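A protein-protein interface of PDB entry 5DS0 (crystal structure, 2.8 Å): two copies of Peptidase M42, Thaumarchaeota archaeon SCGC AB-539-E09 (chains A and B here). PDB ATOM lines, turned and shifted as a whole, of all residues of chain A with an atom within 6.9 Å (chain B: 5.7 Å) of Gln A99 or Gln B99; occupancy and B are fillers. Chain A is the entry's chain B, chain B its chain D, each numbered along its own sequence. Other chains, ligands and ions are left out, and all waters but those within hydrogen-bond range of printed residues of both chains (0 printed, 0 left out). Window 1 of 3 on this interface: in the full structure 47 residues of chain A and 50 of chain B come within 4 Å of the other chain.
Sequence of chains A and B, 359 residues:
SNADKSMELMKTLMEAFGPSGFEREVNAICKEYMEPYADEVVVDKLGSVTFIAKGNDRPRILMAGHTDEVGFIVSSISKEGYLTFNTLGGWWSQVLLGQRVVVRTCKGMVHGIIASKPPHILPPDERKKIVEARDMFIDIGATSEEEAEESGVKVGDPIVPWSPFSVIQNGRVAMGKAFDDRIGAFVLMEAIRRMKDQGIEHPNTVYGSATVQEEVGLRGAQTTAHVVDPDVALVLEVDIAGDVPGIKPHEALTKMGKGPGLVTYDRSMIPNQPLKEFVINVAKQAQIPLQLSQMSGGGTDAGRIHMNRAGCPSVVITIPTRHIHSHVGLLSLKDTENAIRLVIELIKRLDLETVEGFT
O of Leu A97 is in hydrogen-bond range of NE2 of Gln B99, at 3.4 Å.
The backbone carbonyl oxygen (O) of Gly A98 is in hydrogen-bond range of the side-chain amide nitrogen (NE2) of Gln B99 (3.2 Å).
The side-chain amide nitrogen of Gln A99 lies within hydrogen-bond range of the backbone carbonyl oxygen of Leu B97 (3.4 Å).
The side-chain amide nitrogen (NE2) of Gln A99 sits at hydrogen-bond distance from the backbone carbonyl oxygen (O) of Gly B98 (3.2 Å).
The backbone NH (N) of Gly A98 sits at hydrogen-bond distance from the backbone carbonyl oxygen (O) of Ile A114, 3.0 Å away.
O of Arg A100 sits at hydrogen-bond distance from N of Trp A162 (3.0 Å).
The side-chain hydroxyl of Ser A326 is in hydrogen-bond range of the backbone carbonyl oxygen of Val A328, 3.2 Å away.
The backbone NH (N) of Gly B98 sits at hydrogen-bond distance from the backbone carbonyl oxygen (O) of Ile B114, at 3.0 Å.
The backbone carbonyl oxygen (O) of Arg B100 lies within hydrogen-bond range of a ring nitrogen (NE2) of His B327 (2.9 Å).
The backbone NH (N) of Val B101 lies within hydrogen-bond range of the backbone carbonyl oxygen (O) of Gly B112 (2.9 Å).
Among the printed residues, pairs that only touch across the chains: Gln A94 with Leu B97 (3.3 Å), Val A95 with Leu B97 (3.7 Å), Leu A97 with Val B95 (3.7 Å), Gly A98 with Val B328 (3.5 Å), Gln A99 with Gln B99 (3.5 Å), Arg A100 with Val B328 (3.9 Å), Ile A113 with Val B328 (3.8 Å), Met A175 with Arg B100 (3.5 Å), Met A175 with Gly B112 (3.96 Å), Met A175 with Ile B113 (3.7 Å), Val A328 with Gly B98 (3.5 Å), Val A328 with Arg B100 (3.9 Å) and Val A328 with Ile B113 (3.7 Å).
Printed residues of chain B within 4 Å of Gln A94: Leu B97.
Of chain B, only Leu B97, Gly B98 and Gln B99 come within 4 Å of Gln A99.
His A327 touches none of the printed residues of chain B.
Gln B99 touches three residues of chain A.
Printed residues of chain A within 4 Å of Ile B113: Met A175 (3.7 Å) and Val A328 (3.7 Å).
Ile B114 touches none of the printed residues of chain A.
The nearest residue of chain B that does not touch Gln A99 is Val B328 (5.2 Å).
The nearest residue of chain A that does not touch Gln B99 is Val A328 (5.1 Å).
Printed residues of chain B that touch a printed residue of chain A: Val B95, Leu B97, Gly B98, Gln B99, Arg B100, Gly B112, Ile B113 and Val B328.
Hydrophobic or aromatic side chains of chain B within 4 Å of the printed part of chain A: Leu B97, Ile B113 and Val B328.
Among the printed residues, 17 pairs touch across the chains.
Among the printed residues, no Asp or Glu carboxylate lies within 4 Å of a Lys or Arg side-chain nitrogen of the other chain.
Val A95 touches Leu B97, and with the chains exchanged Leu A97 touches Val B95.
Gly A98 touches Val B328, and with the chains exchanged Val A328 touches Gly B98.
Gln B99 touches its own counterpart, Gln A99.
Ile A113 touches Val B328, and with the chains exchanged Val A328 touches Ile B113.
12 positions are printed for both chains.
Of the 17 pairs that touch across the chains among the printed residues, 13 have their exchanged pair printed and touching as well.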
ATOM      1  N   TRP A  91     -25.199  33.053 -38.099  1.00  0.00           N
ATOM      2  CA  TRP A  91     -24.839  33.156 -36.688  1.00  0.00           C
ATOM      3  C   TRP A  91     -24.089  34.453 -36.441  1.00  0.00           C
ATOM      4  O   TRP A  91     -23.320  34.886 -37.270  1.00  0.00           O
ATOM      5  CB  TRP A  91     -23.882  32.047 -36.309  1.00  0.00           C
ATOM      6  CG  TRP A  91     -24.482  30.717 -36.110  1.00  0.00           C
ATOM      7  CD1 TRP A  91     -24.600  29.723 -37.028  1.00  0.00           C
ATOM      8  CD2 TRP A  91     -24.980  30.194 -34.885  1.00  0.00           C
ATOM      9  NE1 TRP A  91     -25.163  28.615 -36.454  1.00  0.00           N
ATOM     10  CE2 TRP A  91     -25.402  28.879 -35.133  1.00  0.00           C
ATOM     11  CE3 TRP A  91     -25.116  30.713 -33.594  1.00  0.00           C
ATOM     12  CZ2 TRP A  91     -25.962  28.076 -34.135  1.00  0.00           C
ATOM     13  CZ3 TRP A  91     -25.672  29.907 -32.610  1.00  0.00           C
ATOM     14  CH2 TRP A  91     -26.085  28.613 -32.883  1.00  0.00           C
ATOM     15  N   GLN A  94     -20.407  36.674 -31.888  1.00  0.00           N
ATOM     16  CA  GLN A  94     -20.292  37.035 -30.475  1.00  0.00           C
ATOM     17  C   GLN A  94     -21.092  36.168 -29.491  1.00  0.00           C
ATOM     18  O   GLN A  94     -20.839  36.225 -28.283  1.00  0.00           O
ATOM     19  CB  GLN A  94     -20.620  38.505 -30.301  1.00  0.00           C
ATOM     20  CG  GLN A  94     -19.707  39.380 -31.154  1.00  0.00           C
ATOM     21  CD  GLN A  94     -19.459  40.753 -30.556  1.00  0.00           C
ATOM     22  OE1 GLN A  94     -19.242  40.878 -29.350  1.00  0.00           O
ATOM     23  NE2 GLN A  94     -19.516  41.785 -31.382  1.00  0.00           N
ATOM     24  N   VAL A  95     -22.015  35.351 -30.002  1.00  0.00           N
ATOM     25  CA  VAL A  95     -22.747  34.384 -29.165  1.00  0.00           C
ATOM     26  C   VAL A  95     -22.182  32.966 -29.173  1.00  0.00           C
ATOM     27  O   VAL A  95     -22.779  32.066 -28.591  1.00  0.00           O
ATOM     28  CB  VAL A  95     -24.246  34.292 -29.544  1.00  0.00           C
ATOM     29  CG1 VAL A  95     -24.933  35.641 -29.413  1.00  0.00           C
ATOM     30  CG2 VAL A  95     -24.442  33.738 -30.945  1.00  0.00           C
ATOM     31  N   LEU A  96     -21.041  32.754 -29.818  1.00  0.00           N
ATOM     32  CA  LEU A  96     -20.517  31.401 -30.025  1.00  0.00           C
ATOM     33  C   LEU A  96     -19.528  30.921 -28.987  1.00  0.00           C
ATOM     34  O   LEU A  96     -19.626  29.805 -28.517  1.00  0.00           O
ATOM     35  CB  LEU A  96     -19.863  31.309 -31.408  1.00  0.00           C
ATOM     36  CG  LEU A  96     -20.790  31.434 -32.629  1.00  0.00           C
ATOM     37  CD1 LEU A  96     -19.967  31.410 -33.902  1.00  0.00           C
ATOM     38  CD2 LEU A  96     -21.835  30.313 -32.653  1.00  0.00           C
ATOM     39  N   LEU A  97     -18.527  31.726 -28.679  1.00  0.00           N
ATOM     40  CA  LEU A  97     -17.465  31.294 -27.770  1.00  0.00           C
ATOM     41  C   LEU A  97     -17.997  30.765 -26.441  1.00  0.00           C
ATOM     42  O   LEU A  97     -18.858  31.390 -25.810  1.00  0.00           O
ATOM     43  CB  LEU A  97     -16.491  32.436 -27.490  1.00  0.00           C
ATOM     44  CG  LEU A  97     -15.377  32.620 -28.508  1.00  0.00           C
ATOM     45  CD1 LEU A  97     -14.397  33.680 -28.022  1.00  0.00           C
ATOM     46  CD2 LEU A  97     -14.638  31.309 -28.768  1.00  0.00           C
ATOM     47  N   GLY A  98     -17.456  29.620 -26.030  1.00  0.00           N
ATOM     48  CA  GLY A  98     -17.729  29.047 -24.730  1.00  0.00           C
ATOM     49  C   GLY A  98     -18.952  28.171 -24.710  1.00  0.00           C
ATOM     50  O   GLY A  98     -19.361  27.718 -23.636  1.00  0.00           O
ATOM     51  N   GLN A  99     -19.553  27.944 -25.876  1.00  0.00           N
ATOM     52  CA  GLN A  99     -20.852  27.285 -25.950  1.00  0.00           C
ATOM     53  C   GLN A  99     -20.733  25.810 -26.202  1.00  0.00           C
ATOM     54  O   GLN A  99     -19.830  25.372 -26.903  1.00  0.00           O
ATOM     55  CB  GLN A  99     -21.696  27.918 -27.051  1.00  0.00           C
ATOM     56  CG  GLN A  99     -22.053  29.380 -26.805  1.00  0.00           C
ATOM     57  CD  GLN A  99     -23.244  29.576 -25.893  1.00  0.00           C
ATOM     58  OE1 GLN A  99     -23.885  28.608 -25.429  1.00  0.00           O
ATOM     59  NE2 GLN A  99     -23.591  30.829 -25.659  1.00  0.00           N
ATOM     60  N   ARG A 100     -21.656  25.045 -25.644  1.00  0.00           N
ATOM     61  CA  ARG A 100     -21.640  23.601 -25.824  1.00  0.00           C
ATOM     62  C   ARG A 100     -22.319  23.216 -27.118  1.00  0.00           C
ATOM     63  O   ARG A 100     -23.395  23.722 -27.441  1.00  0.00           O
ATOM     64  CB  ARG A 100     -22.372  22.903 -24.697  1.00  0.00           C
ATOM     65  CG  ARG A 100     -21.781  23.105 -23.323  1.00  0.00           C
ATOM     66  CD  ARG A 100     -22.884  22.916 -22.302  1.00  0.00           C
ATOM     67  NE  ARG A 100     -22.446  22.875 -20.907  1.00  0.00           N
ATOM     68  CZ  ARG A 100     -22.138  21.770 -20.235  1.00  0.00           C
ATOM     69  NH1 ARG A 100     -22.173  20.589 -20.839  1.00  0.00           N
ATOM     70  NH2 ARG A 100     -21.783  21.849 -18.956  1.00  0.00           N
ATOM     71  N   VAL A 101     -21.721  22.279 -27.835  1.00  0.00           N
ATOM     72  CA  VAL A 101     -22.317  21.753 -29.035  1.00  0.00           C
ATOM     73  C   VAL A 101     -22.271  20.242 -28.972  1.00  0.00           C
ATOM     74  O   VAL A 101     -21.583  19.662 -28.144  1.00  0.00           O
ATOM     75  CB  VAL A 101     -21.574  22.240 -30.295  1.00  0.00           C
ATOM     76  CG1 VAL A 101     -21.725  23.748 -30.454  1.00  0.00           C
ATOM     77  CG2 VAL A 101     -20.095  21.843 -30.260  1.00  0.00           C
ATOM     78  N   GLY A 112     -18.884  18.658 -27.300  1.00  0.00           N
ATOM     79  CA  GLY A 112     -17.756  19.557 -27.421  1.00  0.00           C
ATOM     80  C   GLY A 112     -18.086  20.984 -27.038  1.00  0.00           C
ATOM     81  O   GLY A 112     -19.226  21.315 -26.724  1.00  0.00           O
ATOM     82  N   ILE A 113     -17.066  21.832 -27.097  1.00  0.00           N
ATOM     83  CA  ILE A 113     -17.165  23.221 -26.681  1.00  0.00           C
ATOM     84  C   ILE A 113     -16.548  24.102 -27.738  1.00  0.00           C
ATOM     85  O   ILE A 113     -15.458  23.810 -28.227  1.00  0.00           O
ATOM     86  CB  ILE A 113     -16.360  23.451 -25.413  1.00  0.00           C
ATOM     87  CG1 ILE A 113     -16.846  22.539 -24.303  1.00  0.00           C
ATOM     88  CG2 ILE A 113     -16.481  24.886 -24.972  1.00  0.00           C
ATOM     89  CD1 ILE A 113     -15.874  22.436 -23.151  1.00  0.00           C
ATOM     90  N   ILE A 114     -17.224  25.187 -28.093  1.00  0.00           N
ATOM     91  CA  ILE A 114     -16.657  26.132 -29.053  1.00  0.00           C
ATOM     92  C   ILE A 114     -15.565  26.912 -28.335  1.00  0.00           C
ATOM     93  O   ILE A 114     -15.788  27.464 -27.259  1.00  0.00           O
ATOM     94  CB  ILE A 114     -17.713  27.072 -29.637  1.00  0.00           C
ATOM     95  CG1 ILE A 114     -18.759  26.270 -30.401  1.00  0.00           C
ATOM     96  CG2 ILE A 114     -17.066  28.056 -30.578  1.00  0.00           C
ATOM     97  CD1 ILE A 114     -19.909  27.096 -30.937  1.00  0.00           C
ATOM     98  N   ALA A 115     -14.383  26.954 -28.935  1.00  0.00           N
ATOM     99  CA  ALA A 115     -13.228  27.577 -28.291  1.00  0.00           C
ATOM    100  C   ALA A 115     -12.386  28.379 -29.270  1.00  0.00           C
ATOM    101  O   ALA A 115     -12.527  28.243 -30.490  1.00  0.00           O
ATOM    102  CB  ALA A 115     -12.376  26.510 -27.637  1.00  0.00           C
ATOM    103  N   ILE A 138     -13.825  23.561 -32.282  1.00  0.00           N
ATOM    104  CA  ILE A 138     -14.582  22.808 -31.317  1.00  0.00           C
ATOM    105  C   ILE A 138     -13.649  21.843 -30.616  1.00  0.00           C
ATOM    106  O   ILE A 138     -12.893  21.116 -31.254  1.00  0.00           O
ATOM    107  CB  ILE A 138     -15.738  22.074 -31.996  1.00  0.00           C
ATOM    108  CG1 ILE A 138     -16.775  23.102 -32.413  1.00  0.00           C
ATOM    109  CG2 ILE A 138     -16.374  21.060 -31.067  1.00  0.00           C
ATOM    110  CD1 ILE A 138     -17.596  22.645 -33.584  1.00  0.00           C
ATOM    111  N   PRO A 161     -26.252  23.127 -31.562  1.00  0.00           N
ATOM    112  CA  PRO A 161     -26.145  23.605 -30.196  1.00  0.00           C
ATOM    113  C   PRO A 161     -26.695  22.599 -29.202  1.00  0.00           C
ATOM    114  O   PRO A 161     -27.606  21.849 -29.529  1.00  0.00           O
ATOM    115  CB  PRO A 161     -27.020  24.848 -30.188  1.00  0.00           C
ATOM    116  CG  PRO A 161     -27.136  25.260 -31.601  1.00  0.00           C
ATOM    117  CD  PRO A 161     -27.097  24.002 -32.392  1.00  0.00           C
ATOM    118  N   TRP A 162     -26.115  22.566 -28.009  1.00  0.00           N
ATOM    119  CA  TRP A 162     -26.640  21.755 -26.916  1.00  0.00           C
ATOM    120  C   TRP A 162     -27.427  22.685 -26.006  1.00  0.00           C
ATOM    121  O   TRP A 162     -26.855  23.611 -25.432  1.00  0.00           O
ATOM    122  CB  TRP A 162     -25.511  21.087 -26.125  1.00  0.00           C
ATOM    123  CG  TRP A 162     -26.027  20.154 -25.063  1.00  0.00           C
ATOM    124  CD1 TRP A 162     -26.404  18.854 -25.227  1.00  0.00           C
ATOM    125  CD2 TRP A 162     -26.243  20.467 -23.682  1.00  0.00           C
ATOM    126  NE1 TRP A 162     -26.840  18.332 -24.027  1.00  0.00           N
ATOM    127  CE2 TRP A 162     -26.755  19.300 -23.064  1.00  0.00           C
ATOM    128  CE3 TRP A 162     -26.078  21.627 -22.914  1.00  0.00           C
ATOM    129  CZ2 TRP A 162     -27.092  19.254 -21.714  1.00  0.00           C
ATOM    130  CZ3 TRP A 162     -26.411  21.582 -21.565  1.00  0.00           C
ATOM    131  CH2 TRP A 162     -26.913  20.399 -20.980  1.00  0.00           C
ATOM    132  N   MET A 175     -38.113  27.964 -22.809  1.00  0.00           N
ATOM    133  CA  MET A 175     -36.699  28.253 -22.938  1.00  0.00           C
ATOM    134  C   MET A 175     -36.019  27.090 -23.580  1.00  0.00           C
ATOM    135  O   MET A 175     -36.157  25.962 -23.128  1.00  0.00           O
ATOM    136  CB  MET A 175     -36.093  28.463 -21.562  1.00  0.00           C
ATOM    137  CG  MET A 175     -34.620  28.868 -21.605  1.00  0.00           C
ATOM    138  SD  MET A 175     -34.035  29.268 -19.760  1.00  0.00           S
ATOM    139  CE  MET A 175     -32.130  29.686 -19.939  1.00  0.00           C
ATOM    140  N   SER A 326     -29.389  31.557 -31.799  1.00  0.00           N
ATOM    141  CA  SER A 326     -28.439  31.442 -30.698  1.00  0.00           C
ATOM    142  C   SER A 326     -28.753  30.159 -29.913  1.00  0.00           C
ATOM    143  O   SER A 326     -29.739  29.491 -30.192  1.00  0.00           O
ATOM    144  CB  SER A 326     -28.478  32.709 -29.819  1.00  0.00           C
ATOM    145  OG  SER A 326     -29.350  32.588 -28.705  1.00  0.00           O
ATOM    146  N   HIS A 327     -27.919  29.808 -28.944  1.00  0.00           N
ATOM    147  CA  HIS A 327     -28.116  28.548 -28.211  1.00  0.00           C
ATOM    148  C   HIS A 327     -29.410  28.464 -27.447  1.00  0.00           C
ATOM    149  O   HIS A 327     -30.001  27.401 -27.334  1.00  0.00           O
ATOM    150  CB  HIS A 327     -26.973  28.295 -27.241  1.00  0.00           C
ATOM    151  CG  HIS A 327     -25.811  27.630 -27.879  1.00  0.00           C
ATOM    152  ND1 HIS A 327     -25.131  28.187 -28.937  1.00  0.00           N
ATOM    153  CD2 HIS A 327     -25.235  26.429 -27.644  1.00  0.00           C
ATOM    154  CE1 HIS A 327     -24.169  27.366 -29.317  1.00  0.00           C
ATOM    155  NE2 HIS A 327     -24.212  26.291 -28.549  1.00  0.00           N
ATOM    156  N   VAL A 328     -29.873  29.587 -26.933  1.00  0.00           N
ATOM    157  CA  VAL A 328     -31.062  29.568 -26.113  1.00  0.00           C
ATOM    158  C   VAL A 328     -31.903  30.822 -26.340  1.00  0.00           C
ATOM    159  O   VAL A 328     -31.401  31.936 -26.328  1.00  0.00           O
ATOM    160  CB  VAL A 328     -30.671  29.333 -24.629  1.00  0.00           C
ATOM    161  CG1 VAL A 328     -29.645  30.342 -24.144  1.00  0.00           C
ATOM    162  CG2 VAL A 328     -31.891  29.344 -23.732  1.00  0.00           C
ATOM    163  N   VAL B  95     -16.823  35.381 -24.046  1.00  0.00           N
ATOM    164  CA  VAL B  95     -17.458  34.117 -23.667  1.00  0.00           C
ATOM    165  C   VAL B  95     -18.813  34.256 -22.960  1.00  0.00           C
ATOM    166  O   VAL B  95     -19.375  33.250 -22.525  1.00  0.00           O
ATOM    167  CB  VAL B  95     -16.550  33.241 -22.761  1.00  0.00           C
ATOM    168  CG1 VAL B  95     -15.251  32.910 -23.453  1.00  0.00           C
ATOM    169  CG2 VAL B  95     -16.292  33.897 -21.413  1.00  0.00           C
ATOM    170  N   LEU B  96     -19.332  35.467 -22.848  1.00  0.00           N
ATOM    171  CA  LEU B  96     -20.531  35.709 -22.053  1.00  0.00           C
ATOM    172  C   LEU B  96     -21.847  35.674 -22.810  1.00  0.00           C
ATOM    173  O   LEU B  96     -22.794  35.067 -22.365  1.00  0.00           O
ATOM    174  CB  LEU B  96     -20.412  37.068 -21.357  1.00  0.00           C
ATOM    175  CG  LEU B  96     -19.328  37.199 -20.288  1.00  0.00           C
ATOM    176  CD1 LEU B  96     -19.292  38.632 -19.784  1.00  0.00           C
ATOM    177  CD2 LEU B  96     -19.579  36.238 -19.131  1.00  0.00           C
ATOM    178  N   LEU B  97     -21.929  36.379 -23.928  1.00  0.00           N
ATOM    179  CA  LEU B  97     -23.183  36.467 -24.676  1.00  0.00           C
ATOM    180  C   LEU B  97     -23.791  35.108 -24.990  1.00  0.00           C
ATOM    181  O   LEU B  97     -23.105  34.191 -25.456  1.00  0.00           O
ATOM    182  CB  LEU B  97     -22.995  37.235 -25.988  1.00  0.00           C
ATOM    183  CG  LEU B  97     -23.075  38.750 -25.890  1.00  0.00           C
ATOM    184  CD1 LEU B  97     -23.032  39.356 -27.283  1.00  0.00           C
ATOM    185  CD2 LEU B  97     -24.331  39.195 -25.182  1.00  0.00           C
ATOM    186  N   GLY B  98     -25.095  35.009 -24.742  1.00  0.00           N
ATOM    187  CA  GLY B  98     -25.883  33.834 -25.103  1.00  0.00           C
ATOM    188  C   GLY B  98     -25.848  32.742 -24.070  1.00  0.00           C
ATOM    189  O   GLY B  98     -26.397  31.669 -24.294  1.00  0.00           O
ATOM    190  N   GLN B  99     -25.217  33.012 -22.931  1.00  0.00           N
ATOM    191  CA  GLN B  99     -24.972  31.991 -21.932  1.00  0.00           C
ATOM    192  C   GLN B  99     -26.039  31.957 -20.848  1.00  0.00           C
ATOM    193  O   GLN B  99     -26.571  32.986 -20.465  1.00  0.00           O
ATOM    194  CB  GLN B  99     -23.614  32.207 -21.278  1.00  0.00           C
ATOM    195  CG  GLN B  99     -22.441  32.067 -22.227  1.00  0.00           C
ATOM    196  CD  GLN B  99     -22.003  30.638 -22.463  1.00  0.00           C
ATOM    197  OE1 GLN B  99     -22.548  29.692 -21.893  1.00  0.00           O
ATOM    198  NE2 GLN B  99     -20.998  30.474 -23.295  1.00  0.00           N
ATOM    199  N   ARG B 100     -26.317  30.766 -20.333  1.00  0.00           N
ATOM    200  CA  ARG B 100     -27.312  30.596 -19.287  1.00  0.00           C
ATOM    201  C   ARG B 100     -26.707  30.854 -17.921  1.00  0.00           C
ATOM    202  O   ARG B 100     -25.615  30.387 -17.619  1.00  0.00           O
ATOM    203  CB  ARG B 100     -27.867  29.180 -19.291  1.00  0.00           C
ATOM    204  CG  ARG B 100     -28.569  28.760 -20.566  1.00  0.00           C
ATOM    205  CD  ARG B 100     -28.475  27.263 -20.668  1.00  0.00           C
ATOM    206  NE  ARG B 100     -29.282  26.663 -21.733  1.00  0.00           N
ATOM    207  CZ  ARG B 100     -30.531  26.214 -21.589  1.00  0.00           C
ATOM    208  NH1 ARG B 100     -31.168  26.344 -20.431  1.00  0.00           N
ATOM    209  NH2 ARG B 100     -31.151  25.652 -22.620  1.00  0.00           N
ATOM    210  N   VAL B 101     -27.435  31.590 -17.094  1.00  0.00           N
ATOM    211  CA  VAL B 101     -27.014  31.852 -15.733  1.00  0.00           C
ATOM    212  C   VAL B 101     -28.188  31.586 -14.810  1.00  0.00           C
ATOM    213  O   VAL B 101     -29.313  31.372 -15.261  1.00  0.00           O
ATOM    214  CB  VAL B 101     -26.566  33.296 -15.533  1.00  0.00           C
ATOM    215  CG1 VAL B 101     -25.316  33.588 -16.347  1.00  0.00           C
ATOM    216  CG2 VAL B 101     -27.690  34.265 -15.894  1.00  0.00           C
ATOM    217  N   GLY B 112     -31.858  32.621 -16.227  1.00  0.00           N
ATOM    218  CA  GLY B 112     -31.787  33.691 -17.190  1.00  0.00           C
ATOM    219  C   GLY B 112     -30.713  33.474 -18.235  1.00  0.00           C
ATOM    220  O   GLY B 112     -29.957  32.500 -18.194  1.00  0.00           O
ATOM    221  N   ILE B 113     -30.628  34.430 -19.150  1.00  0.00           N
ATOM    222  CA  ILE B 113     -29.714  34.366 -20.268  1.00  0.00           C
ATOM    223  C   ILE B 113     -28.978  35.685 -20.384  1.00  0.00           C
ATOM    224  O   ILE B 113     -29.608  36.741 -20.337  1.00  0.00           O
ATOM    225  CB  ILE B 113     -30.492  34.179 -21.569  1.00  0.00           C
ATOM    226  CG1 ILE B 113     -31.330  32.916 -21.511  1.00  0.00           C
ATOM    227  CG2 ILE B 113     -29.538  34.089 -22.745  1.00  0.00           C
ATOM    228  CD1 ILE B 113     -32.392  32.858 -22.581  1.00  0.00           C
ATOM    229  N   ILE B 114     -27.662  35.640 -20.584  1.00  0.00           N
ATOM    230  CA  ILE B 114     -26.910  36.860 -20.813  1.00  0.00           C
ATOM    231  C   ILE B 114     -27.209  37.349 -22.226  1.00  0.00           C
ATOM    232  O   ILE B 114     -27.121  36.599 -23.196  1.00  0.00           O
ATOM    233  CB  ILE B 114     -25.409  36.649 -20.629  1.00  0.00           C
ATOM    234  CG1 ILE B 114     -25.123  36.219 -19.198  1.00  0.00           C
ATOM    235  CG2 ILE B 114     -24.662  37.936 -20.928  1.00  0.00           C
ATOM    236  CD1 ILE B 114     -23.669  35.890 -18.927  1.00  0.00           C
ATOM    237  N   HIS B 327     -18.057  29.264 -18.772  1.00  0.00           N
ATOM    238  CA  HIS B 327     -19.159  28.388 -18.359  1.00  0.00           C
ATOM    239  C   HIS B 327     -18.793  26.922 -18.278  1.00  0.00           C
ATOM    240  O   HIS B 327     -19.309  26.200 -17.431  1.00  0.00           O
ATOM    241  CB  HIS B 327     -20.364  28.540 -19.284  1.00  0.00           C
ATOM    242  CG  HIS B 327     -21.247  29.677 -18.907  1.00  0.00           C
ATOM    243  ND1 HIS B 327     -20.801  30.980 -18.880  1.00  0.00           N
ATOM    244  CD2 HIS B 327     -22.538  29.709 -18.502  1.00  0.00           C
ATOM    245  CE1 HIS B 327     -21.780  31.765 -18.471  1.00  0.00           C
ATOM    246  NE2 HIS B 327     -22.844  31.019 -18.233  1.00  0.00           N
ATOM    247  N   VAL B 328     -17.921  26.466 -19.157  1.00  0.00           N
ATOM    248  CA  VAL B 328     -17.620  25.058 -19.210  1.00  0.00           C
ATOM    249  C   VAL B 328     -16.151  24.830 -19.556  1.00  0.00           C
ATOM    250  O   VAL B 328     -15.609  25.422 -20.474  1.00  0.00           O
ATOM    251  CB  VAL B 328     -18.600  24.333 -20.167  1.00  0.00           C
ATOM    252  CG1 VAL B 328     -18.625  24.969 -21.541  1.00  0.00           C
ATOM    253  CG2 VAL B 328     -18.272  22.853 -20.273  1.00  0.00           C
